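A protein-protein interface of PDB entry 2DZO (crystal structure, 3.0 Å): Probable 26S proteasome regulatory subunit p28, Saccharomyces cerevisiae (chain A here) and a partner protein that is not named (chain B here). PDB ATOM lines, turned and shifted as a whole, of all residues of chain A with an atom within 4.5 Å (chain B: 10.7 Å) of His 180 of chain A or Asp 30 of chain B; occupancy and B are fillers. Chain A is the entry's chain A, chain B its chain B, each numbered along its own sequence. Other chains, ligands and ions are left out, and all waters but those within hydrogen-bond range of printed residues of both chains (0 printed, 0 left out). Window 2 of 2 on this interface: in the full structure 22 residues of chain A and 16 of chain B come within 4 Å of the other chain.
Hydrophobic or aromatic side chains of chain A within 4 Å of the printed part of chain B: His 180.
Of the 17 printed residues of chain B, 4 touch a printed residue of chain A.
Among the printed residues, 9 pairs touch across the chains.
Ile 27 of chain B touches Ser 149 of chain A (CD1 to OG, 2.8 Å).
Gln 173 of chain A touches Asp 30 of chain B (NE2 to N, 3.98 Å).
His 180 of chain A touches Ile 27 of chain B.
OE2 of Glu 184 of chain A touches CG1 of Ile 27 of chain B (3.9 Å).
Glu 184 of chain A touches Asp 30 of chain B.
Printed residues of chain B within 4 Å of Gln 141 of chain A: Ile 27 (3.4 Å).
No residue of chain B comes within 4 Å of His 145 of chain A.
Of chain B, only Ile 27 (2.8 Å) comes within 4 Å of Ser 149 of chain A.
No residue of chain B comes within 4 Å of Trp 175 of chain A.
No residue of chain B comes within 4 Å of Pro 177 of chain A.
Phe 179 of chain A touches none of the printed residues of chain B.
No residue of chain B comes within 4 Å of Ala 183 of chain A.
Of the printed residues of chain A, Ile 27 of chain B touches Gln 141, Ser 149, His 180 and Glu 184.
Of the printed residues of chain A, Arg 28 of chain B touches Gln 173.
Of the printed residues of chain A, Asn 29 of chain B touches Gln 173 (3.0 Å).
Of the printed residues of chain A, Asp 30 of chain B touches Gln 173, His 180 and Glu 184.
Tyr 65 of chain B touches none of the printed residues of chain A.
The nearest printed residue of chain A that does not touch Asp 30 of chain B is Ser 149 of chain A (4.1 Å).
O of Ile 27 of chain B lies close to NE2 of Gln 141 of chain A (3.5 Å).
OE1 of Gln 173 of chain A sits close to O of Asn 29 of chain B (3.0 Å).
A ring nitrogen (ND1) of His 180 of chain A lies within hydrogen-bond range of the side-chain carboxylate of Asp 30 of chain B (3.5 Å).
The side-chain amide nitrogen (NE2) of Gln 173 of chain A sits at hydrogen-bond distance from the backbone carbonyl oxygen (O) of Arg 28 of chain B (2.9 Å).
The side-chain carboxylate (OD2) of Asp 171 of chain A lies within hydrogen-bond range of a ring nitrogen (NE2) of His 180 of chain A, 2.6 Å away.
The side-chain amide nitrogen of Gln 141 of chain A sits at hydrogen-bond distance from a ring nitrogen (NE2) of His 180 of chain A (3.4 Å).
The backbone carbonyl oxygen of Ser 24 of chain B is in hydrogen-bond range of the guanidinium group of Arg 28 of chain B, 3.0 Å away.
The backbone carbonyl oxygen (O) of Asn 29 of chain B lies close to the side-chain hydroxyl (OG) of Ser 31 of chain B (3.2 Å).
The side-chain hydroxyl (OG) of Ser 149 of chain A is in hydrogen-bond range of the side-chain carboxylate (OE2) of Glu 184 of chain A.
The side-chain amide oxygen (OD1) of Asn 29 of chain B lies within hydrogen-bond range of the side-chain hydroxyl (OH) of Tyr 65 of chain B, 2.7 Å away.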
ATOM      1  N   GLN A 141      19.977  18.964 -17.615  1.00  0.00           N
ATOM      2  CA  GLN A 141      21.381  18.565 -17.619  1.00  0.00           C
ATOM      3  C   GLN A 141      21.613  17.085 -17.390  1.00  0.00           C
ATOM      4  O   GLN A 141      21.027  16.483 -16.484  1.00  0.00           O
ATOM      5  CB  GLN A 141      22.168  19.359 -16.565  1.00  0.00           C
ATOM      6  CG  GLN A 141      22.169  20.856 -16.791  1.00  0.00           C
ATOM      7  CD  GLN A 141      23.219  21.599 -15.976  1.00  0.00           C
ATOM      8  OE1 GLN A 141      23.196  21.576 -14.745  1.00  0.00           O
ATOM      9  NE2 GLN A 141      24.141  22.274 -16.666  1.00  0.00           N
ATOM     10  N   HIS A 145      27.147  16.855 -19.230  1.00  0.00           N
ATOM     11  CA  HIS A 145      27.187  18.292 -19.021  1.00  0.00           C
ATOM     12  C   HIS A 145      28.128  18.496 -17.872  1.00  0.00           C
ATOM     13  O   HIS A 145      28.952  19.407 -17.888  1.00  0.00           O
ATOM     14  CB  HIS A 145      25.823  18.851 -18.634  1.00  0.00           C
ATOM     15  CG  HIS A 145      24.972  19.235 -19.801  1.00  0.00           C
ATOM     16  ND1 HIS A 145      23.924  18.456 -20.249  1.00  0.00           N
ATOM     17  CD2 HIS A 145      25.024  20.309 -20.625  1.00  0.00           C
ATOM     18  CE1 HIS A 145      23.371  19.034 -21.300  1.00  0.00           C
ATOM     19  NE2 HIS A 145      24.019  20.159 -21.549  1.00  0.00           N
ATOM     20  N   ALA A 148      31.871  17.529 -18.933  1.00  0.00           N
ATOM     21  CA  ALA A 148      32.497  18.543 -19.769  1.00  0.00           C
ATOM     22  C   ALA A 148      32.791  19.759 -18.911  1.00  0.00           C
ATOM     23  O   ALA A 148      33.863  20.355 -19.007  1.00  0.00           O
ATOM     24  CB  ALA A 148      31.573  18.925 -20.923  1.00  0.00           C
ATOM     25  N   SER A 149      31.836  20.120 -18.059  1.00  0.00           N
ATOM     26  CA  SER A 149      31.999  21.275 -17.189  1.00  0.00           C
ATOM     27  C   SER A 149      33.335  21.212 -16.463  1.00  0.00           C
ATOM     28  O   SER A 149      34.099  22.178 -16.497  1.00  0.00           O
ATOM     29  CB  SER A 149      30.863  21.349 -16.181  1.00  0.00           C
ATOM     30  OG  SER A 149      30.863  22.615 -15.551  1.00  0.00           O
ATOM     31  N   ASP A 171      20.938  22.480 -21.911  1.00  0.00           N
ATOM     32  CA  ASP A 171      20.262  22.738 -20.658  1.00  0.00           C
ATOM     33  C   ASP A 171      19.310  23.919 -20.795  1.00  0.00           C
ATOM     34  O   ASP A 171      19.013  24.364 -21.907  1.00  0.00           O
ATOM     35  CB  ASP A 171      21.281  23.011 -19.542  1.00  0.00           C
ATOM     36  CG  ASP A 171      22.369  23.972 -19.964  1.00  0.00           C
ATOM     37  OD1 ASP A 171      22.071  24.902 -20.736  1.00  0.00           O
ATOM     38  OD2 ASP A 171      23.523  23.802 -19.512  1.00  0.00           O
ATOM     39  N   GLN A 173      19.766  27.070 -19.645  1.00  0.00           N
ATOM     40  CA  GLN A 173      20.521  28.214 -20.132  1.00  0.00           C
ATOM     41  C   GLN A 173      20.782  28.039 -21.639  1.00  0.00           C
ATOM     42  O   GLN A 173      21.314  28.933 -22.306  1.00  0.00           O
ATOM     43  CB  GLN A 173      21.836  28.284 -19.363  1.00  0.00           C
ATOM     44  CG  GLN A 173      22.609  29.570 -19.503  1.00  0.00           C
ATOM     45  CD  GLN A 173      23.946  29.502 -18.773  1.00  0.00           C
ATOM     46  OE1 GLN A 173      24.662  30.510 -18.651  1.00  0.00           O
ATOM     47  NE2 GLN A 173      24.295  28.305 -18.286  1.00  0.00           N
ATOM     48  N   TRP A 175      22.683  25.461 -23.044  1.00  0.00           N
ATOM     49  CA  TRP A 175      24.089  25.078 -23.219  1.00  0.00           C
ATOM     50  C   TRP A 175      24.355  23.602 -23.470  1.00  0.00           C
ATOM     51  O   TRP A 175      23.918  22.754 -22.702  1.00  0.00           O
ATOM     52  CB  TRP A 175      24.881  25.478 -21.973  1.00  0.00           C
ATOM     53  CG  TRP A 175      25.332  26.885 -21.955  1.00  0.00           C
ATOM     54  CD1 TRP A 175      24.702  27.959 -22.509  1.00  0.00           C
ATOM     55  CD2 TRP A 175      26.494  27.391 -21.306  1.00  0.00           C
ATOM     56  NE1 TRP A 175      25.402  29.109 -22.247  1.00  0.00           N
ATOM     57  CE2 TRP A 175      26.507  28.789 -21.504  1.00  0.00           C
ATOM     58  CE3 TRP A 175      27.529  26.800 -20.570  1.00  0.00           C
ATOM     59  CZ2 TRP A 175      27.519  29.612 -20.990  1.00  0.00           C
ATOM     60  CZ3 TRP A 175      28.537  27.615 -20.059  1.00  0.00           C
ATOM     61  CH2 TRP A 175      28.522  29.007 -20.273  1.00  0.00           C
ATOM     62  N   THR A 176      25.089  23.290 -24.528  1.00  0.00           N
ATOM     63  CA  THR A 176      25.414  21.900 -24.801  1.00  0.00           C
ATOM     64  C   THR A 176      26.589  21.558 -23.896  1.00  0.00           C
ATOM     65  O   THR A 176      27.164  22.445 -23.269  1.00  0.00           O
ATOM     66  CB  THR A 176      25.821  21.694 -26.265  1.00  0.00           C
ATOM     67  OG1 THR A 176      26.702  22.747 -26.665  1.00  0.00           O
ATOM     68  CG2 THR A 176      24.597  21.692 -27.165  1.00  0.00           C
ATOM     69  N   PRO A 177      26.953  20.269 -23.790  1.00  0.00           N
ATOM     70  CA  PRO A 177      28.088  19.968 -22.916  1.00  0.00           C
ATOM     71  C   PRO A 177      29.335  20.730 -23.343  1.00  0.00           C
ATOM     72  O   PRO A 177      30.242  20.959 -22.538  1.00  0.00           O
ATOM     73  CB  PRO A 177      28.232  18.454 -23.059  1.00  0.00           C
ATOM     74  CG  PRO A 177      26.820  18.016 -23.182  1.00  0.00           C
ATOM     75  CD  PRO A 177      26.257  19.028 -24.179  1.00  0.00           C
ATOM     76  N   LEU A 178      29.359  21.130 -24.611  1.00  0.00           N
ATOM     77  CA  LEU A 178      30.482  21.868 -25.173  1.00  0.00           C
ATOM     78  C   LEU A 178      30.646  23.287 -24.622  1.00  0.00           C
ATOM     79  O   LEU A 178      31.758  23.691 -24.296  1.00  0.00           O
ATOM     80  CB  LEU A 178      30.360  21.935 -26.693  1.00  0.00           C
ATOM     81  CG  LEU A 178      31.466  22.788 -27.310  1.00  0.00           C
ATOM     82  CD1 LEU A 178      32.814  22.133 -27.024  1.00  0.00           C
ATOM     83  CD2 LEU A 178      31.237  22.942 -28.797  1.00  0.00           C
ATOM     84  N   PHE A 179      29.556  24.050 -24.544  1.00  0.00           N
ATOM     85  CA  PHE A 179      29.640  25.400 -24.005  1.00  0.00           C
ATOM     86  C   PHE A 179      30.346  25.248 -22.677  1.00  0.00           C
ATOM     87  O   PHE A 179      31.433  25.774 -22.487  1.00  0.00           O
ATOM     88  CB  PHE A 179      28.261  26.014 -23.761  1.00  0.00           C
ATOM     89  CG  PHE A 179      27.589  26.560 -25.002  1.00  0.00           C
ATOM     90  CD1 PHE A 179      26.645  27.587 -24.895  1.00  0.00           C
ATOM     91  CD2 PHE A 179      27.842  26.022 -26.256  1.00  0.00           C
ATOM     92  CE1 PHE A 179      25.957  28.066 -26.015  1.00  0.00           C
ATOM     93  CE2 PHE A 179      27.158  26.494 -27.387  1.00  0.00           C
ATOM     94  CZ  PHE A 179      26.212  27.517 -27.261  1.00  0.00           C
ATOM     95  N   HIS A 180      29.737  24.506 -21.763  1.00  0.00           N
ATOM     96  CA  HIS A 180      30.329  24.277 -20.450  1.00  0.00           C
ATOM     97  C   HIS A 180      31.835  24.008 -20.515  1.00  0.00           C
ATOM     98  O   HIS A 180      32.627  24.725 -19.904  1.00  0.00           O
ATOM     99  CB  HIS A 180      29.607  23.116 -19.742  1.00  0.00           C
ATOM    100  CG  HIS A 180      28.236  23.476 -19.261  1.00  0.00           C
ATOM    101  ND1 HIS A 180      28.023  24.354 -18.219  1.00  0.00           N
ATOM    102  CD2 HIS A 180      27.010  23.149 -19.731  1.00  0.00           C
ATOM    103  CE1 HIS A 180      26.725  24.557 -18.072  1.00  0.00           C
ATOM    104  NE2 HIS A 180      26.087  23.838 -18.978  1.00  0.00           N
ATOM    105  N   ALA A 181      32.236  22.989 -21.262  1.00  0.00           N
ATOM    106  CA  ALA A 181      33.652  22.669 -21.360  1.00  0.00           C
ATOM    107  C   ALA A 181      34.432  23.694 -22.184  1.00  0.00           C
ATOM    108  O   ALA A 181      35.402  23.355 -22.863  1.00  0.00           O
ATOM    109  CB  ALA A 181      33.826  21.293 -21.946  1.00  0.00           C
ATOM    110  N   LEU A 182      33.999  24.947 -22.136  1.00  0.00           N
ATOM    111  CA  LEU A 182      34.679  26.017 -22.850  1.00  0.00           C
ATOM    112  C   LEU A 182      34.577  27.262 -22.015  1.00  0.00           C
ATOM    113  O   LEU A 182      35.468  28.103 -22.033  1.00  0.00           O
ATOM    114  CB  LEU A 182      34.056  26.287 -24.219  1.00  0.00           C
ATOM    115  CG  LEU A 182      34.611  25.529 -25.423  1.00  0.00           C
ATOM    116  CD1 LEU A 182      34.141  26.231 -26.686  1.00  0.00           C
ATOM    117  CD2 LEU A 182      36.123  25.499 -25.384  1.00  0.00           C
ATOM    118  N   ALA A 183      33.475  27.390 -21.290  1.00  0.00           N
ATOM    119  CA  ALA A 183      33.288  28.543 -20.434  1.00  0.00           C
ATOM    120  C   ALA A 183      34.261  28.340 -19.282  1.00  0.00           C
ATOM    121  O   ALA A 183      34.829  29.293 -18.760  1.00  0.00           O
ATOM    122  CB  ALA A 183      31.857  28.604 -19.934  1.00  0.00           C
ATOM    123  N   GLU A 184      34.451  27.080 -18.895  1.00  0.00           N
ATOM    124  CA  GLU A 184      35.379  26.740 -17.824  1.00  0.00           C
ATOM    125  C   GLU A 184      36.719  26.481 -18.484  1.00  0.00           C
ATOM    126  O   GLU A 184      37.685  26.087 -17.847  1.00  0.00           O
ATOM    127  CB  GLU A 184      34.872  25.524 -17.038  1.00  0.00           C
ATOM    128  CG  GLU A 184      33.540  25.829 -16.331  1.00  0.00           C
ATOM    129  CD  GLU A 184      33.415  25.213 -14.937  1.00  0.00           C
ATOM    130  OE1 GLU A 184      34.396  25.263 -14.163  1.00  0.00           O
ATOM    131  OE2 GLU A 184      32.325  24.698 -14.601  1.00  0.00           O
ATOM    132  N   LEU B  22      28.271  21.242  -4.513  1.00  0.00           N
ATOM    133  CA  LEU B  22      28.290  22.651  -4.845  1.00  0.00           C
ATOM    134  C   LEU B  22      28.474  22.869  -6.345  1.00  0.00           C
ATOM    135  O   LEU B  22      28.067  23.907  -6.883  1.00  0.00           O
ATOM    136  CB  LEU B  22      29.423  23.339  -4.098  1.00  0.00           C
ATOM    137  CG  LEU B  22      29.420  24.864  -4.068  1.00  0.00           C
ATOM    138  CD1 LEU B  22      28.123  25.339  -3.452  1.00  0.00           C
ATOM    139  CD2 LEU B  22      30.602  25.365  -3.278  1.00  0.00           C
ATOM    140  N   ASP B  23      29.051  21.883  -7.033  1.00  0.00           N
ATOM    141  CA  ASP B  23      29.313  21.999  -8.478  1.00  0.00           C
ATOM    142  C   ASP B  23      28.034  22.187  -9.250  1.00  0.00           C
ATOM    143  O   ASP B  23      27.921  22.974 -10.192  1.00  0.00           O
ATOM    144  CB  ASP B  23      30.065  20.762  -9.011  1.00  0.00           C
ATOM    145  CG  ASP B  23      30.221  19.653  -7.974  1.00  0.00           C
ATOM    146  OD1 ASP B  23      30.416  19.970  -6.793  1.00  0.00           O
ATOM    147  OD2 ASP B  23      30.164  18.480  -8.380  1.00  0.00           O
ATOM    148  N   SER B  24      27.057  21.418  -8.835  1.00  0.00           N
ATOM    149  CA  SER B  24      25.763  21.484  -9.455  1.00  0.00           C
ATOM    150  C   SER B  24      25.316  22.950  -9.441  1.00  0.00           C
ATOM    151  O   SER B  24      24.854  23.508 -10.444  1.00  0.00           O
ATOM    152  CB  SER B  24      24.771  20.655  -8.660  1.00  0.00           C
ATOM    153  OG  SER B  24      24.539  21.272  -7.421  1.00  0.00           O
ATOM    154  N   LEU B  25      25.483  23.578  -8.286  1.00  0.00           N
ATOM    155  CA  LEU B  25      25.063  24.954  -8.065  1.00  0.00           C
ATOM    156  C   LEU B  25      25.724  26.006  -8.944  1.00  0.00           C
ATOM    157  O   LEU B  25      25.082  26.978  -9.324  1.00  0.00           O
ATOM    158  CB  LEU B  25      25.247  25.295  -6.580  1.00  0.00           C
ATOM    159  CG  LEU B  25      24.089  26.083  -5.949  1.00  0.00           C
ATOM    160  CD1 LEU B  25      24.227  26.128  -4.452  1.00  0.00           C
ATOM    161  CD2 LEU B  25      24.026  27.493  -6.494  1.00  0.00           C
ATOM    162  N   ILE B  26      26.996  25.804  -9.265  1.00  0.00           N
ATOM    163  CA  ILE B  26      27.733  26.742 -10.102  1.00  0.00           C
ATOM    164  C   ILE B  26      27.429  26.537 -11.600  1.00  0.00           C
ATOM    165  O   ILE B  26      27.239  27.487 -12.362  1.00  0.00           O
ATOM    166  CB  ILE B  26      29.263  26.587  -9.879  1.00  0.00           C
ATOM    167  CG1 ILE B  26      29.670  25.144 -10.206  1.00  0.00           C
ATOM    168  CG2 ILE B  26      29.631  26.843  -8.411  1.00  0.00           C
ATOM    169  CD1 ILE B  26      31.139  24.915 -10.625  1.00  0.00           C
ATOM    170  N   ILE B  27      27.362  25.271 -11.991  1.00  0.00           N
ATOM    171  CA  ILE B  27      27.143  24.853 -13.365  1.00  0.00           C
ATOM    172  C   ILE B  27      25.797  25.186 -13.998  1.00  0.00           C
ATOM    173  O   ILE B  27      25.620  25.047 -15.208  1.00  0.00           O
ATOM    174  CB  ILE B  27      27.447  23.344 -13.477  1.00  0.00           C
ATOM    175  CG1 ILE B  27      28.964  23.157 -13.475  1.00  0.00           C
ATOM    176  CG2 ILE B  27      26.841  22.755 -14.716  1.00  0.00           C
ATOM    177  CD1 ILE B  27      29.434  21.725 -13.309  1.00  0.00           C
ATOM    178  N   ARG B  28      24.851  25.659 -13.199  1.00  0.00           N
ATOM    179  CA  ARG B  28      23.539  26.006 -13.735  1.00  0.00           C
ATOM    180  C   ARG B  28      23.619  27.114 -14.766  1.00  0.00           C
ATOM    181  O   ARG B  28      23.440  26.859 -15.957  1.00  0.00           O
ATOM    182  CB  ARG B  28      22.595  26.362 -12.594  1.00  0.00           C
ATOM    183  CG  ARG B  28      22.384  25.141 -11.743  1.00  0.00           C
ATOM    184  CD  ARG B  28      21.954  25.412 -10.331  1.00  0.00           C
ATOM    185  NE  ARG B  28      22.126  24.194  -9.544  1.00  0.00           N
ATOM    186  CZ  ARG B  28      21.575  23.982  -8.356  1.00  0.00           C
ATOM    187  NH1 ARG B  28      20.802  24.910  -7.806  1.00  0.00           N
ATOM    188  NH2 ARG B  28      21.803  22.841  -7.719  1.00  0.00           N
ATOM    189  N   ASN B  29      23.898  28.340 -14.344  1.00  0.00           N
ATOM    190  CA  ASN B  29      24.006  29.400 -15.334  1.00  0.00           C
ATOM    191  C   ASN B  29      25.406  29.986 -15.406  1.00  0.00           C
ATOM    192  O   ASN B  29      25.582  31.129 -15.824  1.00  0.00           O
ATOM    193  CB  ASN B  29      22.979  30.509 -15.084  1.00  0.00           C
ATOM    194  CG  ASN B  29      23.227  31.256 -13.800  1.00  0.00           C
ATOM    195  OD1 ASN B  29      23.034  30.722 -12.702  1.00  0.00           O
ATOM    196  ND2 ASN B  29      23.661  32.507 -13.926  1.00  0.00           N
ATOM    197  N   ASP B  30      26.390  29.182 -15.012  1.00  0.00           N
ATOM    198  CA  ASP B  30      27.804  29.565 -15.036  1.00  0.00           C
ATOM    199  C   ASP B  30      28.065  31.030 -15.392  1.00  0.00           C
ATOM    200  O   ASP B  30      28.680  31.330 -16.420  1.00  0.00           O
ATOM    201  CB  ASP B  30      28.573  28.679 -16.029  1.00  0.00           C
ATOM    202  CG  ASP B  30      29.423  27.619 -15.343  1.00  0.00           C
ATOM    203  OD1 ASP B  30      30.158  27.975 -14.389  1.00  0.00           O
ATOM    204  OD2 ASP B  30      29.364  26.440 -15.769  1.00  0.00           O
ATOM    205  N   SER B  31      27.601  31.937 -14.540  1.00  0.00           N
ATOM    206  CA  SER B  31      27.780  33.367 -14.769  1.00  0.00           C
ATOM    207  C   SER B  31      27.288  34.143 -13.546  1.00  0.00           C
ATOM    208  O   SER B  31      26.412  35.009 -13.650  1.00  0.00           O
ATOM    209  CB  SER B  31      27.012  33.811 -16.026  1.00  0.00           C
ATOM    210  OG  SER B  31      27.577  33.269 -17.214  1.00  0.00           O
ATOM    211  N   LEU B  32      27.864  33.820 -12.391  1.00  0.00           N
ATOM    212  CA  LEU B  32      27.493  34.460 -11.135  1.00  0.00           C
ATOM    213  C   LEU B  32      28.570  35.369 -10.548  1.00  0.00           C
ATOM    214  O   LEU B  32      29.737  34.987 -10.438  1.00  0.00           O
ATOM    215  CB  LEU B  32      27.118  33.398 -10.103  1.00  0.00           C
ATOM    216  CG  LEU B  32      25.635  33.177  -9.832  1.00  0.00           C
ATOM    217  CD1 LEU B  32      25.480  32.118  -8.757  1.00  0.00           C
ATOM    218  CD2 LEU B  32      24.995  34.488  -9.386  1.00  0.00           C
ATOM    219  N   SER B  33      28.156  36.573 -10.165  1.00  0.00           N
ATOM    220  CA  SER B  33      29.054  37.556  -9.579  1.00  0.00           C
ATOM    221  C   SER B  33      29.564  37.008  -8.262  1.00  0.00           C
ATOM    222  O   SER B  33      28.775  36.565  -7.423  1.00  0.00           O
ATOM    223  CB  SER B  33      28.308  38.854  -9.304  1.00  0.00           C
ATOM    224  OG  SER B  33      27.469  38.709  -8.169  1.00  0.00           O
ATOM    225  N   GLY B  34      30.880  37.051  -8.080  1.00  0.00           N
ATOM    226  CA  GLY B  34      31.479  36.551  -6.857  1.00  0.00           C
ATOM    227  C   GLY B  34      30.723  36.930  -5.594  1.00  0.00           C
ATOM    228  O   GLY B  34      30.801  36.221  -4.585  1.00  0.00           O
ATOM    229  N   ILE B  37      27.774  34.561  -4.840  1.00  0.00           N
ATOM    230  CA  ILE B  37      28.364  33.331  -4.338  1.00  0.00           C
ATOM    231  C   ILE B  37      28.509  33.477  -2.826  1.00  0.00           C
ATOM    232  O   ILE B  37      28.152  32.585  -2.072  1.00  0.00           O
ATOM    233  CB  ILE B  37      29.757  33.066  -4.976  1.00  0.00           C
ATOM    234  CG1 ILE B  37      29.921  33.876  -6.267  1.00  0.00           C
ATOM    235  CG2 ILE B  37      29.912  31.594  -5.317  1.00  0.00           C
ATOM    236  CD1 ILE B  37      28.907  33.591  -7.331  1.00  0.00           C
ATOM    237  N   ILE B  40      24.962  33.434  -1.396  1.00  0.00           N
ATOM    238  CA  ILE B  40      24.467  32.082  -1.507  1.00  0.00           C
ATOM    239  C   ILE B  40      25.130  31.267  -0.406  1.00  0.00           C
ATOM    240  O   ILE B  40      24.456  30.662   0.424  1.00  0.00           O
ATOM    241  CB  ILE B  40      24.871  31.467  -2.854  1.00  0.00           C
ATOM    242  CG1 ILE B  40      24.103  32.148  -3.981  1.00  0.00           C
ATOM    243  CG2 ILE B  40      24.641  29.971  -2.838  1.00  0.00           C
ATOM    244  CD1 ILE B  40      24.582  31.746  -5.347  1.00  0.00           C
ATOM    245  N   TYR B  65      20.613  29.160  -3.017  1.00  0.00           N
ATOM    246  CA  TYR B  65      20.660  29.559  -4.417  1.00  0.00           C
ATOM    247  C   TYR B  65      19.373  30.300  -4.765  1.00  0.00           C
ATOM    248  O   TYR B  65      19.404  31.373  -5.354  1.00  0.00           O
ATOM    249  CB  TYR B  65      20.810  28.313  -5.291  1.00  0.00           C
ATOM    250  CG  TYR B  65      21.055  28.573  -6.760  1.00  0.00           C
ATOM    251  CD1 TYR B  65      22.030  29.479  -7.173  1.00  0.00           C
ATOM    252  CD2 TYR B  65      20.362  27.858  -7.737  1.00  0.00           C
ATOM    253  CE1 TYR B  65      22.319  29.664  -8.519  1.00  0.00           C
ATOM    254  CE2 TYR B  65      20.641  28.036  -9.090  1.00  0.00           C
ATOM    255  CZ  TYR B  65      21.623  28.943  -9.474  1.00  0.00           C
ATOM    256  OH  TYR B  65      21.912  29.138 -10.807  1.00  0.00           O
ATOM    257  N   VAL B  69      19.533  34.581  -6.152  1.00  0.00           N
ATOM    258  CA  VAL B  69      19.874  34.842  -7.539  1.00  0.00           C
ATOM    259  C   VAL B  69      18.921  35.788  -8.264  1.00  0.00           C
ATOM    260  O   VAL B  69      18.799  36.950  -7.879  1.00  0.00           O
ATOM    261  CB  VAL B  69      20.024  33.517  -8.318  1.00  0.00           C
ATOM    262  CG1 VAL B  69      20.567  33.778  -9.718  1.00  0.00           C
ATOM    263  CG2 VAL B  69      20.974  32.606  -7.572  1.00  0.00           C
